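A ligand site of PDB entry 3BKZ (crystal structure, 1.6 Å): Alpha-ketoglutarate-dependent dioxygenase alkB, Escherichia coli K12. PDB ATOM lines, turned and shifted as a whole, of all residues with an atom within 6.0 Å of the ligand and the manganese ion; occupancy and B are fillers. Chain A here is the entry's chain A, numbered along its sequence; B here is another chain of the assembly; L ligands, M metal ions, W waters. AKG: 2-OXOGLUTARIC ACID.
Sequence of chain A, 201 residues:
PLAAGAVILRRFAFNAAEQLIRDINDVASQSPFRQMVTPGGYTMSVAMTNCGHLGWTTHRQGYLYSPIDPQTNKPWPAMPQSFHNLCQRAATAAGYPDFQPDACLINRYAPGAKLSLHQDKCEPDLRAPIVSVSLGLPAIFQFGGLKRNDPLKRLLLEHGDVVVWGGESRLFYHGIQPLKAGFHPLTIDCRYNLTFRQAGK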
ATOM      1  N   LEU A 105     -22.178  30.226   4.370  1.00  0.00           N
ATOM      2  CA  LEU A 105     -21.593  29.181   3.532  1.00  0.00           C
ATOM      3  C   LEU A 105     -22.337  27.866   3.780  1.00  0.00           C
ATOM      4  O   LEU A 105     -22.538  27.470   4.924  1.00  0.00           O
ATOM      5  CB  LEU A 105     -20.109  29.022   3.853  1.00  0.00           C
ATOM      6  CG  LEU A 105     -19.295  27.906   3.204  1.00  0.00           C
ATOM      7  CD1 LEU A 105     -19.245  28.073   1.701  1.00  0.00           C
ATOM      8  CD2 LEU A 105     -17.896  27.907   3.784  1.00  0.00           C
ATOM      9  N   ASN A 107     -21.939  23.993   3.195  1.00  0.00           N
ATOM     10  CA  ASN A 107     -21.006  22.914   2.863  1.00  0.00           C
ATOM     11  C   ASN A 107     -21.741  21.584   2.774  1.00  0.00           C
ATOM     12  O   ASN A 107     -22.559  21.275   3.655  1.00  0.00           O
ATOM     13  CB  ASN A 107     -19.913  22.792   3.929  1.00  0.00           C
ATOM     14  CG  ASN A 107     -19.037  24.024   4.018  1.00  0.00           C
ATOM     15  OD1 ASN A 107     -18.848  24.578   5.107  1.00  0.00           O
ATOM     16  ND2 ASN A 107     -18.497  24.446   2.888  1.00  0.00           N
ATOM     17  N   TYR A 109     -20.903  17.488   2.527  1.00  0.00           N
ATOM     18  CA  TYR A 109     -19.913  16.440   2.654  1.00  0.00           C
ATOM     19  C   TYR A 109     -20.488  15.107   2.193  1.00  0.00           C
ATOM     20  O   TYR A 109     -21.420  14.587   2.806  1.00  0.00           O
ATOM     21  CB  TYR A 109     -19.469  16.293   4.122  1.00  0.00           C
ATOM     22  CG  TYR A 109     -18.721  17.469   4.698  1.00  0.00           C
ATOM     23  CD1 TYR A 109     -19.404  18.631   5.090  1.00  0.00           C
ATOM     24  CD2 TYR A 109     -17.346  17.423   4.873  1.00  0.00           C
ATOM     25  CE1 TYR A 109     -18.711  19.717   5.636  1.00  0.00           C
ATOM     26  CE2 TYR A 109     -16.646  18.503   5.413  1.00  0.00           C
ATOM     27  CZ  TYR A 109     -17.334  19.641   5.790  1.00  0.00           C
ATOM     28  OH  TYR A 109     -16.645  20.704   6.320  1.00  0.00           O
ATOM     29  N   LEU A 115     -12.397  18.576   5.617  1.00  0.00           N
ATOM     30  CA  LEU A 115     -11.923  19.944   5.574  1.00  0.00           C
ATOM     31  C   LEU A 115     -10.687  20.006   6.444  1.00  0.00           C
ATOM     32  O   LEU A 115     -10.772  19.884   7.662  1.00  0.00           O
ATOM     33  CB  LEU A 115     -13.013  20.908   6.031  1.00  0.00           C
ATOM     34  CG  LEU A 115     -12.866  22.385   5.657  1.00  0.00           C
ATOM     35  CD1 LEU A 115     -12.757  22.573   4.157  1.00  0.00           C
ATOM     36  CD2 LEU A 115     -14.049  23.122   6.193  1.00  0.00           C
ATOM     37  N   HIS A 118      -7.643  24.626   9.362  1.00  0.00           N
ATOM     38  CA  HIS A 118      -7.513  25.993   8.874  1.00  0.00           C
ATOM     39  C   HIS A 118      -8.062  26.980   9.901  1.00  0.00           C
ATOM     40  O   HIS A 118      -8.796  26.587  10.817  1.00  0.00           O
ATOM     41  CB  HIS A 118      -8.290  26.160   7.563  1.00  0.00           C
ATOM     42  CG  HIS A 118      -9.768  26.028   7.730  1.00  0.00           C
ATOM     43  ND1 HIS A 118     -10.405  24.799   7.795  1.00  0.00           N
ATOM     44  CD2 HIS A 118     -10.749  26.962   7.881  1.00  0.00           C
ATOM     45  CE1 HIS A 118     -11.703  24.989   7.959  1.00  0.00           C
ATOM     46  NE2 HIS A 118     -11.935  26.287   8.020  1.00  0.00           N
ATOM     47  N   GLN A 119      -7.714  28.254   9.740  1.00  0.00           N
ATOM     48  CA  GLN A 119      -8.331  29.346  10.494  1.00  0.00           C
ATOM     49  C   GLN A 119      -9.297  30.094   9.581  1.00  0.00           C
ATOM     50  O   GLN A 119      -9.045  30.233   8.391  1.00  0.00           O
ATOM     51  CB  GLN A 119      -7.274  30.354  10.960  1.00  0.00           C
ATOM     52  CG  GLN A 119      -6.197  29.804  11.844  1.00  0.00           C
ATOM     53  CD  GLN A 119      -5.095  30.820  12.094  1.00  0.00           C
ATOM     54  OE1 GLN A 119      -4.311  31.130  11.196  1.00  0.00           O
ATOM     55  NE2 GLN A 119      -5.038  31.345  13.314  1.00  0.00           N
ATOM     56  N   ASP A 120     -10.400  30.586  10.161  1.00  0.00           N
ATOM     57  CA  ASP A 120     -11.278  31.528   9.470  1.00  0.00           C
ATOM     58  C   ASP A 120     -10.697  32.917   9.695  1.00  0.00           C
ATOM     59  O   ASP A 120     -10.923  33.510  10.747  1.00  0.00           O
ATOM     60  CB  ASP A 120     -12.701  31.472  10.044  1.00  0.00           C
ATOM     61  CG  ASP A 120     -13.475  30.234   9.617  1.00  0.00           C
ATOM     62  OD1 ASP A 120     -12.890  29.277   9.080  1.00  0.00           O
ATOM     63  OD2 ASP A 120     -14.707  30.243   9.848  1.00  0.00           O
ATOM     64  N   SER A 132     -21.810  27.750  13.478  1.00  0.00           N
ATOM     65  CA  SER A 132     -21.608  26.581  12.614  1.00  0.00           C
ATOM     66  C   SER A 132     -22.648  25.491  12.924  1.00  0.00           C
ATOM     67  O   SER A 132     -22.629  24.908  14.012  1.00  0.00           O
ATOM     68  CB  SER A 132     -20.185  26.048  12.827  1.00  0.00           C
ATOM     69  OG  SER A 132     -19.824  25.109  11.823  1.00  0.00           O
ATOM     70  N   VAL A 133     -23.528  25.219  11.967  1.00  0.00           N
ATOM     71  CA  VAL A 133     -24.644  24.281  12.140  1.00  0.00           C
ATOM     72  C   VAL A 133     -24.407  22.944  11.423  1.00  0.00           C
ATOM     73  O   VAL A 133     -24.088  22.930  10.234  1.00  0.00           O
ATOM     74  CB  VAL A 133     -25.979  24.902  11.634  1.00  0.00           C
ATOM     75  CG1 VAL A 133     -27.171  23.973  11.917  1.00  0.00           C
ATOM     76  CG2 VAL A 133     -26.201  26.278  12.251  1.00  0.00           C
ATOM     77  N   SER A 134     -24.596  21.835  12.147  1.00  0.00           N
ATOM     78  CA  SER A 134     -24.441  20.485  11.575  1.00  0.00           C
ATOM     79  C   SER A 134     -25.790  19.859  11.258  1.00  0.00           C
ATOM     80  O   SER A 134     -26.710  19.912  12.071  1.00  0.00           O
ATOM     81  CB  SER A 134     -23.693  19.578  12.543  1.00  0.00           C
ATOM     82  OG  SER A 134     -22.342  19.960  12.696  1.00  0.00           O
ATOM     83  N   PHE A 141     -15.244  16.754  14.350  1.00  0.00           N
ATOM     84  CA  PHE A 141     -14.800  18.146  14.267  1.00  0.00           C
ATOM     85  C   PHE A 141     -13.529  18.327  15.079  1.00  0.00           C
ATOM     86  O   PHE A 141     -13.479  17.922  16.240  1.00  0.00           O
ATOM     87  CB  PHE A 141     -15.916  19.036  14.814  1.00  0.00           C
ATOM     88  CG  PHE A 141     -15.621  20.510  14.795  1.00  0.00           C
ATOM     89  CD1 PHE A 141     -15.454  21.183  13.585  1.00  0.00           C
ATOM     90  CD2 PHE A 141     -15.570  21.243  15.980  1.00  0.00           C
ATOM     91  CE1 PHE A 141     -15.200  22.554  13.563  1.00  0.00           C
ATOM     92  CE2 PHE A 141     -15.321  22.615  15.972  1.00  0.00           C
ATOM     93  CZ  PHE A 141     -15.140  23.270  14.758  1.00  0.00           C
ATOM     94  N   LEU A 157     -19.863  15.741  15.906  1.00  0.00           N
ATOM     95  CA  LEU A 157     -20.983  16.639  15.682  1.00  0.00           C
ATOM     96  C   LEU A 157     -22.088  15.868  14.998  1.00  0.00           C
ATOM     97  O   LEU A 157     -21.889  15.287  13.923  1.00  0.00           O
ATOM     98  CB  LEU A 157     -20.582  17.842  14.821  1.00  0.00           C
ATOM     99  CG  LEU A 157     -19.446  18.732  15.335  1.00  0.00           C
ATOM    100  CD1 LEU A 157     -19.219  19.896  14.393  1.00  0.00           C
ATOM    101  CD2 LEU A 157     -19.730  19.237  16.748  1.00  0.00           C
ATOM    102  N   TRP A 165     -17.826  29.912  17.902  1.00  0.00           N
ATOM    103  CA  TRP A 165     -16.566  30.404  18.453  1.00  0.00           C
ATOM    104  C   TRP A 165     -16.344  31.878  18.124  1.00  0.00           C
ATOM    105  O   TRP A 165     -16.851  32.388  17.133  1.00  0.00           O
ATOM    106  CB  TRP A 165     -15.369  29.511  18.101  1.00  0.00           C
ATOM    107  CG  TRP A 165     -15.040  29.345  16.637  1.00  0.00           C
ATOM    108  CD1 TRP A 165     -14.057  29.990  15.941  1.00  0.00           C
ATOM    109  CD2 TRP A 165     -15.649  28.427  15.707  1.00  0.00           C
ATOM    110  NE1 TRP A 165     -14.030  29.559  14.634  1.00  0.00           N
ATOM    111  CE2 TRP A 165     -14.994  28.601  14.462  1.00  0.00           C
ATOM    112  CE3 TRP A 165     -16.696  27.491  15.805  1.00  0.00           C
ATOM    113  CZ2 TRP A 165     -15.354  27.863  13.324  1.00  0.00           C
ATOM    114  CZ3 TRP A 165     -17.049  26.764  14.662  1.00  0.00           C
ATOM    115  CH2 TRP A 165     -16.374  26.956  13.437  1.00  0.00           C
ATOM    116  N   HIS A 174      -9.339  24.750  13.050  1.00  0.00           N
ATOM    117  CA  HIS A 174     -10.416  23.764  13.118  1.00  0.00           C
ATOM    118  C   HIS A 174     -10.553  23.039  11.781  1.00  0.00           C
ATOM    119  O   HIS A 174     -10.014  23.485  10.769  1.00  0.00           O
ATOM    120  CB  HIS A 174     -11.742  24.436  13.486  1.00  0.00           C
ATOM    121  CG  HIS A 174     -12.138  25.514  12.533  1.00  0.00           C
ATOM    122  ND1 HIS A 174     -11.659  26.802  12.618  1.00  0.00           N
ATOM    123  CD2 HIS A 174     -12.951  25.493  11.444  1.00  0.00           C
ATOM    124  CE1 HIS A 174     -12.165  27.526  11.631  1.00  0.00           C
ATOM    125  NE2 HIS A 174     -12.951  26.761  10.910  1.00  0.00           N
ATOM    126  N   GLY A 175     -11.279  21.929  11.787  1.00  0.00           N
ATOM    127  CA  GLY A 175     -11.516  21.179  10.554  1.00  0.00           C
ATOM    128  C   GLY A 175     -12.466  20.021  10.759  1.00  0.00           C
ATOM    129  O   GLY A 175     -12.983  19.817  11.855  1.00  0.00           O
ATOM    130  N   ILE A 176     -12.688  19.272   9.685  1.00  0.00           N
ATOM    131  CA  ILE A 176     -13.583  18.116   9.693  1.00  0.00           C
ATOM    132  C   ILE A 176     -12.846  16.905   9.103  1.00  0.00           C
ATOM    133  O   ILE A 176     -12.283  16.986   8.009  1.00  0.00           O
ATOM    134  CB  ILE A 176     -14.891  18.387   8.891  1.00  0.00           C
ATOM    135  CG1 ILE A 176     -15.766  19.437   9.604  1.00  0.00           C
ATOM    136  CG2 ILE A 176     -15.656  17.075   8.608  1.00  0.00           C
ATOM    137  CD1 ILE A 176     -16.572  18.933  10.817  1.00  0.00           C
ATOM    138  N   ARG A 191     -23.609  14.962   4.825  1.00  0.00           N
ATOM    139  CA  ARG A 191     -23.669  15.941   5.897  1.00  0.00           C
ATOM    140  C   ARG A 191     -23.719  17.332   5.288  1.00  0.00           C
ATOM    141  O   ARG A 191     -22.957  17.637   4.354  1.00  0.00           O
ATOM    142  CB  ARG A 191     -22.445  15.819   6.811  1.00  0.00           C
ATOM    143  CG  ARG A 191     -22.353  16.914   7.862  1.00  0.00           C
ATOM    144  CD  ARG A 191     -21.136  16.739   8.752  1.00  0.00           C
ATOM    145  NE  ARG A 191     -21.092  17.761   9.797  1.00  0.00           N
ATOM    146  CZ  ARG A 191     -20.365  18.877   9.731  1.00  0.00           C
ATOM    147  NH1 ARG A 191     -19.606  19.112   8.672  1.00  0.00           N
ATOM    148  NH2 ARG A 191     -20.390  19.751  10.720  1.00  0.00           N
ATOM    149  N   ASN A 193     -23.360  21.473   6.364  1.00  0.00           N
ATOM    150  CA  ASN A 193     -22.968  22.435   7.383  1.00  0.00           C
ATOM    151  C   ASN A 193     -23.323  23.844   6.924  1.00  0.00           C
ATOM    152  O   ASN A 193     -23.154  24.171   5.750  1.00  0.00           O
ATOM    153  CB  ASN A 193     -21.478  22.310   7.690  1.00  0.00           C
ATOM    154  CG  ASN A 193     -20.923  23.530   8.398  1.00  0.00           C
ATOM    155  OD1 ASN A 193     -20.403  24.447   7.756  1.00  0.00           O
ATOM    156  ND2 ASN A 193     -21.049  23.566   9.727  1.00  0.00           N
ATOM    157  N   THR A 195     -22.301  27.647   7.757  1.00  0.00           N
ATOM    158  CA  THR A 195     -21.342  28.498   8.455  1.00  0.00           C
ATOM    159  C   THR A 195     -21.706  29.973   8.258  1.00  0.00           C
ATOM    160  O   THR A 195     -21.585  30.504   7.154  1.00  0.00           O
ATOM    161  CB  THR A 195     -19.890  28.208   7.999  1.00  0.00           C
ATOM    162  OG1 THR A 195     -19.519  26.878   8.387  1.00  0.00           O
ATOM    163  CG2 THR A 195     -18.919  29.196   8.631  1.00  0.00           C
ATOM    164  N   ARG A 197     -21.167  33.966   8.978  1.00  0.00           N
ATOM    165  CA  ARG A 197     -20.110  34.921   9.267  1.00  0.00           C
ATOM    166  C   ARG A 197     -20.569  36.358   9.013  1.00  0.00           C
ATOM    167  O   ARG A 197     -21.491  36.586   8.226  1.00  0.00           O
ATOM    168  CB  ARG A 197     -18.856  34.647   8.426  1.00  0.00           C
ATOM    169  CG  ARG A 197     -18.306  33.222   8.508  1.00  0.00           C
ATOM    170  CD  ARG A 197     -16.900  33.112   7.917  1.00  0.00           C
ATOM    171  NE  ARG A 197     -16.419  31.735   7.911  1.00  0.00           N
ATOM    172  CZ  ARG A 197     -16.059  31.050   6.828  1.00  0.00           C
ATOM    173  NH1 ARG A 197     -16.083  31.616   5.628  1.00  0.00           N
ATOM    174  NH2 ARG A 197     -15.633  29.792   6.944  1.00  0.00           N
ATOM    175  P   2YR B   8      -5.479  26.383   4.363  1.00  0.00           P
ATOM    176  OP1 2YR B   8      -5.670  27.704   3.719  1.00  0.00           O
ATOM    177  OP2 2YR B   8      -5.400  26.308   5.845  1.00  0.00           O
ATOM    178  O5' 2YR B   8      -6.626  25.413   3.818  1.00  0.00           O
ATOM    179  C5' 2YR B   8      -6.938  24.158   4.411  1.00  0.00           C
ATOM    180  C4' 2YR B   8      -8.332  23.729   3.958  1.00  0.00           C
ATOM    181  O4' 2YR B   8      -9.311  24.615   4.561  1.00  0.00           O
ATOM    182  C3' 2YR B   8      -8.606  23.805   2.454  1.00  0.00           C
ATOM    183  O3' 2YR B   8      -9.532  22.799   2.050  1.00  0.00           O
ATOM    184  C2' 2YR B   8      -9.245  25.181   2.279  1.00  0.00           C
ATOM    185  C1' 2YR B   8     -10.046  25.296   3.564  1.00  0.00           C
ATOM    186  N1  2YR B   8     -10.280  26.683   4.066  1.00  0.00           N
ATOM    187  C2  2YR B   8     -11.585  27.168   4.245  1.00  0.00           C
ATOM    188  O2  2YR B   8     -12.555  26.441   3.978  1.00  0.00           O
ATOM    189  N3  2YR B   8     -11.761  28.432   4.708  1.00  0.00           N
ATOM    190  C4  2YR B   8     -10.697  29.195   4.995  1.00  0.00           C
ATOM    191  N4  2YR B   8     -10.881  30.436   5.456  1.00  0.00           N
ATOM    192  C5  2YR B   8      -9.368  28.727   4.824  1.00  0.00           C
ATOM    193  C6  2YR B   8      -9.205  27.481   4.364  1.00  0.00           C
ATOM    194  S   2YR B   8     -10.957  33.186   4.061  1.00  0.00           S
ATOM    195  C8  2YR B   8     -11.947  32.615   5.463  1.00  0.00           C
ATOM    196  C9  2YR B   8     -12.178  31.127   5.382  1.00  0.00           C
HETATM  197  C1  AKG L   1     -15.705  26.097   6.959  1.00  0.00           C
HETATM  198  O1  AKG L   1     -16.439  25.882   5.964  1.00  0.00           O
HETATM  199  O2  AKG L   1     -14.874  27.030   6.965  1.00  0.00           O
HETATM  200  C2  AKG L   1     -15.807  25.207   8.112  1.00  0.00           C
HETATM  201  O5  AKG L   1     -14.979  25.290   9.005  1.00  0.00           O
HETATM  202  C3  AKG L   1     -16.935  24.194   8.157  1.00  0.00           C
HETATM  203  C4  AKG L   1     -16.777  23.213   9.317  1.00  0.00           C
HETATM  204  C5  AKG L   1     -17.893  22.187   9.351  1.00  0.00           C
HETATM  205  O3  AKG L   1     -18.309  21.688   8.273  1.00  0.00           O
HETATM  206  O4  AKG L   1     -18.368  21.860  10.462  1.00  0.00           O
HETATM  207 MN    MN M   1     -13.673  27.209   8.917  1.00  0.00          MN
HETATM  208  O   HOH W   1     -15.665  28.020   9.708  1.00  0.00           O
HETATM  209  O   HOH W   2     -17.727  26.497  10.351  1.00  0.00           O
HETATM  210  O   HOH W   3     -18.621  22.914  12.879  1.00  0.00           O
HETATM  211  O   HOH W   4     -14.407  29.063   4.277  1.00  0.00           O
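An oxygen (O3) of the ligand is in hydrogen-bond range of the side-chain hydroxyl of Tyr 109 (2.7 Å).
NH2 of Arg 197 lies close to O2 of the ligand (2.9 Å).
An oxygen (O1) of the ligand sits close to the side-chain amide oxygen (OD1) of Asn 107 (2.9 Å).
The guanidinium group (NH1) of Arg 191 is in salt-bridge range of an oxygen (O3) of the ligand, 2.9 Å away.
An oxygen (O4) of the ligand lies within hydrogen-bond range of the side-chain amide nitrogen (ND2) of Asn 193, at 3.3 Å.
N of Tyr 109 lies within hydrogen-bond range of O of Arg 191, 2.8 Å away.
The backbone carbonyl oxygen of Asn 107 is in hydrogen-bond range of the backbone NH of Asn 193 (2.8 Å).
The side-chain hydroxyl of Ser 134 lies within hydrogen-bond range of the guanidinium group of Arg 191.
OG1 of Thr 195 sits at hydrogen-bond distance from OD1 of Asn 193, 2.7 Å away.
The side-chain amide nitrogen (ND2) of Asn 193 is in hydrogen-bond range of the side-chain hydroxyl (OG) of Ser 132, 2.9 Å away.
O of Val 133 sits close to ND2 of Asn 193, 3.1 Å away.
The backbone carbonyl oxygen (O) of Leu 105 sits at hydrogen-bond distance from the backbone NH (N) of Thr 195.
O of Leu 115 lies within hydrogen-bond range of N of Ile 176.
Residues that only touch the ligand: Leu 105 (3.3 Å), Leu 115 (3.3 Å), Ile 176 (3.5 Å), Thr 195 (3.7 Å), Ser 132 (3.8 Å) and 2YR 8 of chain B (3.8 Å).
14 residues have an atom within 4 Å of the ligand: Leu 105, Asn 107, Tyr 109, Leu 115, His 118, Asp 120, Ser 132, His 174, Ile 176, Arg 191, Asn 193, Thr 195, Arg 197 and 2YR 8 of chain B.
The nearest printed residue that does not touch the ligand is Phe 141 (4.3 Å).
NH2 of Arg 197 touches the manganese ion, at 3.8 Å.
Within 4 Å of the manganese ion: His 118, Asp 120, His 174 and Arg 197.
Along chain A the residues within 4 Å of the manganese ion span positions 118 to 197.
NE2 of His 118 binds the manganese ion.
The manganese ion is bound by NE2 of His 174.
OD1 of Asp 120 binds the manganese ion, 2.2 Å away.
The manganese ion is bound by water W1.
O2 of the ligand binds the manganese ion, 2.3 Å away.
O5 of the ligand is bound to the manganese ion (2.3 Å).
The manganese ion has six donor atoms within binding distance.
Water W1 bridges OD2 of Asp 120 (2.4 Å) and NH2 of Arg 197 (3.3 Å).
Water W3 bridges an oxygen (O4) of the ligand (2.6 Å) and the side-chain hydroxyl (OG) of Ser 132 (2.7 Å).
Water W2 lies within hydrogen-bond range of the side-chain hydroxyl (OG1) of Thr 195 (2.7 Å) and the side-chain hydroxyl (OG) of Ser 132 (2.9 Å).
Water W4 lies within hydrogen-bond range of N3 of 2YR 8 of chain B (2.8 Å) and NH2 of Arg 197 (3.0 Å).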
